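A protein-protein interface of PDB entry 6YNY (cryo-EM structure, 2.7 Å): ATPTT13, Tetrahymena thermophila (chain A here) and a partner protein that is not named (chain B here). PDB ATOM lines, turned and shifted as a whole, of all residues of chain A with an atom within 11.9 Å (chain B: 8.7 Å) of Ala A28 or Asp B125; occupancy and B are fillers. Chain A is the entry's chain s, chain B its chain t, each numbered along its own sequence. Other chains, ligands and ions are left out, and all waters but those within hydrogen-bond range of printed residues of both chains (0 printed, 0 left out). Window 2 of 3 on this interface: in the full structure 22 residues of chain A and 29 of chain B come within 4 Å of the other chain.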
ATOM      1  N   TRP A  24     -12.812   3.348 -38.486  1.00  0.00           N
ATOM      2  CA  TRP A  24     -13.512   2.238 -37.861  1.00  0.00           C
ATOM      3  C   TRP A  24     -14.547   2.669 -36.835  1.00  0.00           C
ATOM      4  O   TRP A  24     -15.372   1.842 -36.433  1.00  0.00           O
ATOM      5  CB  TRP A  24     -12.516   1.287 -37.184  1.00  0.00           C
ATOM      6  CG  TRP A  24     -11.657   0.551 -38.146  1.00  0.00           C
ATOM      7  CD1 TRP A  24     -10.367   0.829 -38.473  1.00  0.00           C
ATOM      8  CD2 TRP A  24     -12.033  -0.589 -38.919  1.00  0.00           C
ATOM      9  NE1 TRP A  24      -9.910  -0.072 -39.401  1.00  0.00           N
ATOM     10  CE2 TRP A  24     -10.917  -0.954 -39.693  1.00  0.00           C
ATOM     11  CE3 TRP A  24     -13.204  -1.340 -39.030  1.00  0.00           C
ATOM     12  CZ2 TRP A  24     -10.938  -2.035 -40.565  1.00  0.00           C
ATOM     13  CZ3 TRP A  24     -13.224  -2.410 -39.894  1.00  0.00           C
ATOM     14  CH2 TRP A  24     -12.098  -2.749 -40.652  1.00  0.00           C
ATOM     15  N   GLY A  25     -14.533   3.923 -36.404  1.00  0.00           N
ATOM     16  CA  GLY A  25     -15.483   4.377 -35.416  1.00  0.00           C
ATOM     17  C   GLY A  25     -15.107   3.905 -34.023  1.00  0.00           C
ATOM     18  O   GLY A  25     -13.946   3.613 -33.718  1.00  0.00           O
ATOM     19  N   SER A  26     -16.119   3.830 -33.166  1.00  0.00           N
ATOM     20  CA  SER A  26     -15.944   3.404 -31.786  1.00  0.00           C
ATOM     21  C   SER A  26     -16.242   1.917 -31.675  1.00  0.00           C
ATOM     22  O   SER A  26     -17.318   1.462 -32.077  1.00  0.00           O
ATOM     23  CB  SER A  26     -16.856   4.200 -30.852  1.00  0.00           C
ATOM     24  OG  SER A  26     -16.665   3.817 -29.503  1.00  0.00           O
ATOM     25  N   LEU A  27     -15.285   1.165 -31.130  1.00  0.00           N
ATOM     26  CA  LEU A  27     -15.497  -0.263 -30.928  1.00  0.00           C
ATOM     27  C   LEU A  27     -16.714  -0.518 -30.051  1.00  0.00           C
ATOM     28  O   LEU A  27     -17.479  -1.457 -30.296  1.00  0.00           O
ATOM     29  CB  LEU A  27     -14.255  -0.888 -30.298  1.00  0.00           C
ATOM     30  CG  LEU A  27     -14.327  -2.384 -29.995  1.00  0.00           C
ATOM     31  CD1 LEU A  27     -14.066  -3.188 -31.248  1.00  0.00           C
ATOM     32  CD2 LEU A  27     -13.359  -2.756 -28.887  1.00  0.00           C
ATOM     33  N   ALA A  28     -16.908   0.303 -29.021  1.00  0.00           N
ATOM     34  CA  ALA A  28     -18.017   0.081 -28.103  1.00  0.00           C
ATOM     35  C   ALA A  28     -19.358   0.265 -28.801  1.00  0.00           C
ATOM     36  O   ALA A  28     -20.251  -0.578 -28.683  1.00  0.00           O
ATOM     37  CB  ALA A  28     -17.902   1.025 -26.911  1.00  0.00           C
ATOM     38  N   GLU A  29     -19.514   1.362 -29.535  1.00  0.00           N
ATOM     39  CA  GLU A  29     -20.786   1.653 -30.176  1.00  0.00           C
ATOM     40  C   GLU A  29     -21.146   0.570 -31.186  1.00  0.00           C
ATOM     41  O   GLU A  29     -20.280  -0.018 -31.839  1.00  0.00           O
ATOM     42  CB  GLU A  29     -20.732   3.012 -30.871  1.00  0.00           C
ATOM     43  CG  GLU A  29     -20.462   4.175 -29.943  1.00  0.00           C
ATOM     44  CD  GLU A  29     -20.370   5.495 -30.677  1.00  0.00           C
ATOM     45  OE1 GLU A  29     -20.407   5.485 -31.926  1.00  0.00           O
ATOM     46  OE2 GLU A  29     -20.261   6.543 -30.008  1.00  0.00           O
ATOM     47  N   ARG A  30     -22.442   0.306 -31.300  1.00  0.00           N
ATOM     48  CA  ARG A  30     -22.956  -0.611 -32.307  1.00  0.00           C
ATOM     49  C   ARG A  30     -23.364   0.188 -33.537  1.00  0.00           C
ATOM     50  O   ARG A  30     -23.307   1.424 -33.518  1.00  0.00           O
ATOM     51  CB  ARG A  30     -24.152  -1.390 -31.772  1.00  0.00           C
ATOM     52  CG  ARG A  30     -23.964  -1.968 -30.403  1.00  0.00           C
ATOM     53  CD  ARG A  30     -25.116  -2.882 -30.073  1.00  0.00           C
ATOM     54  NE  ARG A  30     -25.072  -4.113 -30.850  1.00  0.00           N
ATOM     55  CZ  ARG A  30     -26.108  -4.922 -31.027  1.00  0.00           C
ATOM     56  NH1 ARG A  30     -27.281  -4.631 -30.492  1.00  0.00           N
ATOM     57  NH2 ARG A  30     -25.973  -6.023 -31.746  1.00  0.00           N
ATOM     58  N   PRO A  31     -23.779  -0.466 -34.620  1.00  0.00           N
ATOM     59  CA  PRO A  31     -24.293   0.281 -35.767  1.00  0.00           C
ATOM     60  C   PRO A  31     -25.482   1.143 -35.378  1.00  0.00           C
ATOM     61  O   PRO A  31     -26.263   0.799 -34.490  1.00  0.00           O
ATOM     62  CB  PRO A  31     -24.696  -0.817 -36.753  1.00  0.00           C
ATOM     63  CG  PRO A  31     -23.881  -1.971 -36.383  1.00  0.00           C
ATOM     64  CD  PRO A  31     -23.695  -1.906 -34.907  1.00  0.00           C
ATOM     65  N   MET A  32     -25.612   2.280 -36.060  1.00  0.00           N
ATOM     66  CA  MET A  32     -26.690   3.206 -35.748  1.00  0.00           C
ATOM     67  C   MET A  32     -28.061   2.590 -35.986  1.00  0.00           C
ATOM     68  O   MET A  32     -29.051   3.077 -35.431  1.00  0.00           O
ATOM     69  CB  MET A  32     -26.530   4.479 -36.573  1.00  0.00           C
ATOM     70  CG  MET A  32     -27.528   5.568 -36.238  1.00  0.00           C
ATOM     71  SD  MET A  32     -27.490   6.049 -34.505  1.00  0.00           S
ATOM     72  CE  MET A  32     -25.883   6.821 -34.431  1.00  0.00           C
ATOM     73  N   VAL A  33     -28.141   1.529 -36.791  1.00  0.00           N
ATOM     74  CA  VAL A  33     -29.427   0.884 -37.047  1.00  0.00           C
ATOM     75  C   VAL A  33     -30.001   0.326 -35.755  1.00  0.00           C
ATOM     76  O   VAL A  33     -31.200   0.454 -35.481  1.00  0.00           O
ATOM     77  CB  VAL A  33     -29.285  -0.226 -38.105  1.00  0.00           C
ATOM     78  CG1 VAL A  33     -30.620  -0.502 -38.757  1.00  0.00           C
ATOM     79  CG2 VAL A  33     -28.261   0.132 -39.136  1.00  0.00           C
ATOM     80  N   ASP A  34     -29.156  -0.311 -34.945  1.00  0.00           N
ATOM     81  CA  ASP A  34     -29.623  -0.902 -33.699  1.00  0.00           C
ATOM     82  C   ASP A  34     -30.058   0.160 -32.700  1.00  0.00           C
ATOM     83  O   ASP A  34     -30.882  -0.117 -31.823  1.00  0.00           O
ATOM     84  CB  ASP A  34     -28.520  -1.774 -33.102  1.00  0.00           C
ATOM     85  CG  ASP A  34     -28.065  -2.865 -34.047  1.00  0.00           C
ATOM     86  OD1 ASP A  34     -28.606  -2.946 -35.168  1.00  0.00           O
ATOM     87  OD2 ASP A  34     -27.164  -3.643 -33.670  1.00  0.00           O
ATOM     88  N   ARG A  35     -29.518   1.368 -32.813  1.00  0.00           N
ATOM     89  CA  ARG A  35     -29.834   2.447 -31.889  1.00  0.00           C
ATOM     90  C   ARG A  35     -31.034   3.265 -32.335  1.00  0.00           C
ATOM     91  O   ARG A  35     -31.744   3.824 -31.492  1.00  0.00           O
ATOM     92  CB  ARG A  35     -28.623   3.363 -31.733  1.00  0.00           C
ATOM     93  CG  ARG A  35     -27.413   2.681 -31.139  1.00  0.00           C
ATOM     94  CD  ARG A  35     -26.224   3.609 -31.086  1.00  0.00           C
ATOM     95  NE  ARG A  35     -25.354   3.484 -32.247  1.00  0.00           N
ATOM     96  CZ  ARG A  35     -24.399   4.353 -32.559  1.00  0.00           C
ATOM     97  NH1 ARG A  35     -24.200   5.421 -31.802  1.00  0.00           N
ATOM     98  NH2 ARG A  35     -23.645   4.158 -33.630  1.00  0.00           N
ATOM     99  N   ARG B  95     -20.696  -2.387 -10.803  1.00  0.00           N
ATOM    100  CA  ARG B  95     -20.867  -1.525 -11.966  1.00  0.00           C
ATOM    101  C   ARG B  95     -22.059  -1.958 -12.813  1.00  0.00           C
ATOM    102  O   ARG B  95     -22.966  -1.162 -13.069  1.00  0.00           O
ATOM    103  CB  ARG B  95     -19.589  -1.527 -12.814  1.00  0.00           C
ATOM    104  CG  ARG B  95     -19.660  -0.632 -14.036  1.00  0.00           C
ATOM    105  CD  ARG B  95     -18.369  -0.668 -14.824  1.00  0.00           C
ATOM    106  NE  ARG B  95     -18.075  -2.006 -15.330  1.00  0.00           N
ATOM    107  CZ  ARG B  95     -18.635  -2.535 -16.415  1.00  0.00           C
ATOM    108  NH1 ARG B  95     -18.305  -3.762 -16.798  1.00  0.00           N
ATOM    109  NH2 ARG B  95     -19.528  -1.847 -17.115  1.00  0.00           N
ATOM    110  N   PHE B 119     -30.926  -0.889 -11.981  1.00  0.00           N
ATOM    111  CA  PHE B 119     -30.486  -0.583 -13.335  1.00  0.00           C
ATOM    112  C   PHE B 119     -29.325  -1.494 -13.696  1.00  0.00           C
ATOM    113  O   PHE B 119     -28.361  -1.606 -12.933  1.00  0.00           O
ATOM    114  CB  PHE B 119     -30.069   0.881 -13.462  1.00  0.00           C
ATOM    115  CG  PHE B 119     -29.431   1.217 -14.774  1.00  0.00           C
ATOM    116  CD1 PHE B 119     -30.201   1.431 -15.896  1.00  0.00           C
ATOM    117  CD2 PHE B 119     -28.060   1.325 -14.885  1.00  0.00           C
ATOM    118  CE1 PHE B 119     -29.620   1.740 -17.100  1.00  0.00           C
ATOM    119  CE2 PHE B 119     -27.475   1.635 -16.088  1.00  0.00           C
ATOM    120  CZ  PHE B 119     -28.256   1.844 -17.195  1.00  0.00           C
ATOM    121  N   ARG B 121     -26.464  -2.007 -16.446  1.00  0.00           N
ATOM    122  CA  ARG B 121     -25.770  -1.322 -17.524  1.00  0.00           C
ATOM    123  C   ARG B 121     -25.423  -2.297 -18.642  1.00  0.00           C
ATOM    124  O   ARG B 121     -25.123  -3.469 -18.407  1.00  0.00           O
ATOM    125  CB  ARG B 121     -24.508  -0.650 -16.991  1.00  0.00           C
ATOM    126  CG  ARG B 121     -23.754   0.163 -18.018  1.00  0.00           C
ATOM    127  CD  ARG B 121     -22.406   0.603 -17.490  1.00  0.00           C
ATOM    128  NE  ARG B 121     -21.579   1.183 -18.545  1.00  0.00           N
ATOM    129  CZ  ARG B 121     -20.313   1.556 -18.390  1.00  0.00           C
ATOM    130  NH1 ARG B 121     -19.709   1.414 -17.216  1.00  0.00           N
ATOM    131  NH2 ARG B 121     -19.648   2.075 -19.411  1.00  0.00           N
ATOM    132  N   GLY B 122     -25.462  -1.796 -19.872  1.00  0.00           N
ATOM    133  CA  GLY B 122     -25.146  -2.618 -21.017  1.00  0.00           C
ATOM    134  C   GLY B 122     -23.661  -2.699 -21.296  1.00  0.00           C
ATOM    135  O   GLY B 122     -22.852  -1.924 -20.789  1.00  0.00           O
ATOM    136  N   LYS B 123     -23.306  -3.672 -22.136  1.00  0.00           N
ATOM    137  CA  LYS B 123     -21.908  -3.858 -22.503  1.00  0.00           C
ATOM    138  C   LYS B 123     -21.380  -2.674 -23.300  1.00  0.00           C
ATOM    139  O   LYS B 123     -20.230  -2.260 -23.121  1.00  0.00           O
ATOM    140  CB  LYS B 123     -21.753  -5.141 -23.312  1.00  0.00           C
ATOM    141  CG  LYS B 123     -22.091  -6.400 -22.554  1.00  0.00           C
ATOM    142  CD  LYS B 123     -21.829  -7.638 -23.389  1.00  0.00           C
ATOM    143  CE  LYS B 123     -22.058  -8.894 -22.578  1.00  0.00           C
ATOM    144  NZ  LYS B 123     -21.714 -10.120 -23.337  1.00  0.00           N
ATOM    145  N   TYR B 124     -22.201  -2.127 -24.185  1.00  0.00           N
ATOM    146  CA  TYR B 124     -21.784  -1.084 -25.103  1.00  0.00           C
ATOM    147  C   TYR B 124     -22.195   0.295 -24.600  1.00  0.00           C
ATOM    148  O   TYR B 124     -23.068   0.438 -23.741  1.00  0.00           O
ATOM    149  CB  TYR B 124     -22.364  -1.358 -26.486  1.00  0.00           C
ATOM    150  CG  TYR B 124     -22.074  -2.768 -26.940  1.00  0.00           C
ATOM    151  CD1 TYR B 124     -20.792  -3.149 -27.301  1.00  0.00           C
ATOM    152  CD2 TYR B 124     -23.076  -3.723 -26.985  1.00  0.00           C
ATOM    153  CE1 TYR B 124     -20.519  -4.435 -27.703  1.00  0.00           C
ATOM    154  CE2 TYR B 124     -22.810  -5.013 -27.388  1.00  0.00           C
ATOM    155  CZ  TYR B 124     -21.529  -5.363 -27.747  1.00  0.00           C
ATOM    156  OH  TYR B 124     -21.252  -6.647 -28.150  1.00  0.00           O
ATOM    157  N   ASP B 125     -21.550   1.315 -25.164  1.00  0.00           N
ATOM    158  CA  ASP B 125     -21.681   2.671 -24.641  1.00  0.00           C
ATOM    159  C   ASP B 125     -23.115   3.174 -24.746  1.00  0.00           C
ATOM    160  O   ASP B 125     -23.763   3.459 -23.733  1.00  0.00           O
ATOM    161  CB  ASP B 125     -20.727   3.604 -25.385  1.00  0.00           C
ATOM    162  CG  ASP B 125     -19.275   3.295 -25.102  1.00  0.00           C
ATOM    163  OD1 ASP B 125     -19.008   2.394 -24.280  1.00  0.00           O
ATOM    164  OD2 ASP B 125     -18.400   3.952 -25.703  1.00  0.00           O
ATOM    165  N   ASP B 126     -23.628   3.295 -25.966  1.00  0.00           N
ATOM    166  CA  ASP B 126     -24.947   3.869 -26.207  1.00  0.00           C
ATOM    167  C   ASP B 126     -25.880   2.763 -26.680  1.00  0.00           C
ATOM    168  O   ASP B 126     -25.709   2.225 -27.779  1.00  0.00           O
ATOM    169  CB  ASP B 126     -24.871   5.001 -27.228  1.00  0.00           C
ATOM    170  CG  ASP B 126     -24.110   4.611 -28.471  1.00  0.00           C
ATOM    171  OD1 ASP B 126     -23.334   3.635 -28.408  1.00  0.00           O
ATOM    172  OD2 ASP B 126     -24.282   5.283 -29.509  1.00  0.00           O
ATOM    173  N   LEU B 127     -26.860   2.432 -25.850  1.00  0.00           N
ATOM    174  CA  LEU B 127     -27.866   1.438 -26.172  1.00  0.00           C
ATOM    175  C   LEU B 127     -29.217   1.944 -25.698  1.00  0.00           C
ATOM    176  O   LEU B 127     -29.299   2.632 -24.674  1.00  0.00           O
ATOM    177  CB  LEU B 127     -27.579   0.086 -25.504  1.00  0.00           C
ATOM    178  CG  LEU B 127     -26.304  -0.659 -25.869  1.00  0.00           C
ATOM    179  CD1 LEU B 127     -26.155  -1.865 -24.971  1.00  0.00           C
ATOM    180  CD2 LEU B 127     -26.324  -1.078 -27.316  1.00  0.00           C
ATOM    181  N   PRO B 128     -30.289   1.628 -26.419  1.00  0.00           N
ATOM    182  CA  PRO B 128     -31.622   1.963 -25.917  1.00  0.00           C
ATOM    183  C   PRO B 128     -31.890   1.263 -24.594  1.00  0.00           C
ATOM    184  O   PRO B 128     -31.208   0.310 -24.215  1.00  0.00           O
ATOM    185  CB  PRO B 128     -32.561   1.475 -27.027  1.00  0.00           C
ATOM    186  CG  PRO B 128     -31.742   0.618 -27.902  1.00  0.00           C
ATOM    187  CD  PRO B 128     -30.338   1.047 -27.768  1.00  0.00           C
ATOM    188  N   THR B 129     -32.882   1.768 -23.871  1.00  0.00           N
ATOM    189  CA  THR B 129     -33.178   1.278 -22.536  1.00  0.00           C
ATOM    190  C   THR B 129     -34.414   0.389 -22.546  1.00  0.00           C
ATOM    191  O   THR B 129     -35.325   0.564 -23.359  1.00  0.00           O
ATOM    192  CB  THR B 129     -33.390   2.435 -21.559  1.00  0.00           C
ATOM    193  OG1 THR B 129     -34.457   3.265 -22.023  1.00  0.00           O
ATOM    194  CG2 THR B 129     -32.134   3.259 -21.453  1.00  0.00           C
ATOM    195  N   LEU B 155     -27.979  -7.801 -22.349  1.00  0.00           N
ATOM    196  CA  LEU B 155     -27.425  -6.470 -22.152  1.00  0.00           C
ATOM    197  C   LEU B 155     -26.663  -5.989 -23.375  1.00  0.00           C
ATOM    198  O   LEU B 155     -26.494  -4.777 -23.551  1.00  0.00           O
ATOM    199  CB  LEU B 155     -26.527  -6.454 -20.920  1.00  0.00           C
ATOM    200  CG  LEU B 155     -27.250  -6.745 -19.606  1.00  0.00           C
ATOM    201  CD1 LEU B 155     -26.293  -6.680 -18.451  1.00  0.00           C
ATOM    202  CD2 LEU B 155     -28.395  -5.784 -19.390  1.00  0.00           C
ATOM    203  N   ALA B 156     -26.190  -6.907 -24.216  1.00  0.00           N
ATOM    204  CA  ALA B 156     -25.570  -6.511 -25.472  1.00  0.00           C
ATOM    205  C   ALA B 156     -26.521  -5.712 -26.347  1.00  0.00           C
ATOM    206  O   ALA B 156     -26.066  -4.984 -27.235  1.00  0.00           O
ATOM    207  CB  ALA B 156     -25.092  -7.742 -26.230  1.00  0.00           C
ATOM    208  N   ASN B 159     -29.922  -1.514 -22.290  1.00  0.00           N
ATOM    209  CA  ASN B 159     -29.815  -1.312 -20.856  1.00  0.00           C
ATOM    210  C   ASN B 159     -31.159  -1.594 -20.209  1.00  0.00           C
ATOM    211  O   ASN B 159     -32.208  -1.217 -20.737  1.00  0.00           O
ATOM    212  CB  ASN B 159     -29.360   0.110 -20.548  1.00  0.00           C
ATOM    213  CG  ASN B 159     -27.952   0.379 -21.013  1.00  0.00           C
ATOM    214  OD1 ASN B 159     -27.064  -0.456 -20.859  1.00  0.00           O
ATOM    215  ND2 ASN B 159     -27.738   1.548 -21.590  1.00  0.00           N
ATOM    216  N   HIS B 438     -33.211   8.527 -32.972  1.00  0.00           N
ATOM    217  CA  HIS B 438     -32.338   8.010 -31.932  1.00  0.00           C
ATOM    218  C   HIS B 438     -33.124   7.804 -30.642  1.00  0.00           C
ATOM    219  O   HIS B 438     -34.109   8.495 -30.371  1.00  0.00           O
ATOM    220  CB  HIS B 438     -31.174   8.969 -31.700  1.00  0.00           C
ATOM    221  CG  HIS B 438     -30.001   8.343 -31.017  1.00  0.00           C
ATOM    222  ND1 HIS B 438     -29.898   8.249 -29.647  1.00  0.00           N
ATOM    223  CD2 HIS B 438     -28.875   7.785 -31.518  1.00  0.00           C
ATOM    224  CE1 HIS B 438     -28.761   7.655 -29.333  1.00  0.00           C
ATOM    225  NE2 HIS B 438     -28.121   7.363 -30.450  1.00  0.00           N
ATOM    226  N   HIS B 439     -32.677   6.841 -29.838  1.00  0.00           N
ATOM    227  CA  HIS B 439     -33.472   6.414 -28.694  1.00  0.00           C
ATOM    228  C   HIS B 439     -33.559   7.488 -27.615  1.00  0.00           C
ATOM    229  O   HIS B 439     -34.521   7.496 -26.840  1.00  0.00           O
ATOM    230  CB  HIS B 439     -32.910   5.116 -28.123  1.00  0.00           C
ATOM    231  CG  HIS B 439     -31.483   5.209 -27.688  1.00  0.00           C
ATOM    232  ND1 HIS B 439     -31.107   5.773 -26.490  1.00  0.00           N
ATOM    233  CD2 HIS B 439     -30.342   4.806 -28.291  1.00  0.00           C
ATOM    234  CE1 HIS B 439     -29.792   5.714 -26.374  1.00  0.00           C
ATOM    235  NE2 HIS B 439     -29.305   5.132 -27.453  1.00  0.00           N
ATOM    236  N   ASN B 440     -32.582   8.386 -27.534  1.00  0.00           N
ATOM    237  CA  ASN B 440     -32.582   9.470 -26.555  1.00  0.00           C
ATOM    238  C   ASN B 440     -32.235  10.786 -27.237  1.00  0.00           C
ATOM    239  O   ASN B 440     -31.431  11.580 -26.750  1.00  0.00           O
ATOM    240  CB  ASN B 440     -31.631   9.190 -25.392  1.00  0.00           C
ATOM    241  CG  ASN B 440     -30.185   9.153 -25.817  1.00  0.00           C
ATOM    242  OD1 ASN B 440     -29.871   8.884 -26.974  1.00  0.00           O
ATOM    243  ND2 ASN B 440     -29.288   9.427 -24.878  1.00  0.00           N
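NE of Arg A35 lies within salt-bridge range of OD2 of Asp B126 (3.4 Å).
The guanidinium group of Arg A30 lies within hydrogen-bond range of the backbone carbonyl oxygen of Ala B156.
The guanidinium group of Arg A30 lies within salt-bridge range of the side-chain carboxylate of Asp A34, 3.3 Å away.
A ring nitrogen (ND1) of His B438 sits at hydrogen-bond distance from the side-chain amide oxygen of Asn B440 (2.7 Å).
ND1 of His B439 sits close to OD1 of Asn B440, 3.4 Å away.
The side-chain carboxylate (OE1) of Glu A29 lies within salt-bridge range of the guanidinium group (NH1) of Arg A35 (3.8 Å).
O of Arg A30 lies within hydrogen-bond range of NH2 of Arg A35, 2.8 Å away.
Among the printed residues, merely in contact across the chains: Ala A28 with Tyr B124, Ala A28 with Asp B125, Glu A29 with Asp B126, Arg A30 with Leu B127, Arg A35 with His B439, Met A32 with His B438 and Arg A30 with Tyr B124.
Ala A28 touches just these residues of chain B: Tyr B124 and Asp B125.
No residue of chain A comes within 4 Å of Gly B122.
Of chain A, only Ala A28 (3.0 Å) and Arg A30 (3.8 Å) come within 4 Å of Tyr B124.
Asp B126 touches just these residues of chain A: Glu A29 and Arg A35.
Printed residues of chain A within 4 Å of Leu B127: Arg A30.
Printed residues of chain B within 4 Å of Arg A30: Tyr B124, Leu B127 and Ala B156.
Of the printed residues of chain B, Met A32 touches His B438.
Of the printed residues of chain B, Arg A35 touches Asp B126 (2.3 Å) and His B439 (3.6 Å).
The nearest residue of chain A that does not touch Asp B125 is Ser A26 (4.2 Å).
Hydrophobic or aromatic side chains of chain A that line the printed part of chain B: Ala A28 and Met A32.
Of the 17 printed residues of chain B, 7 touch a printed residue of chain A.
Hydrophobic or aromatic side chains of chain B within 4 Å of the printed part of chain A: Tyr B124, Leu B127, His B438 and His B439.
Along chain B the printed residues that touch a printed residue of chain A span positions 124 to 439.
Among the printed residues, Asp or Glu carboxylates within 4 Å of a Lys or Arg side-chain nitrogen of the other chain: Arg A35 with Asp B126 (2.3 Å).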
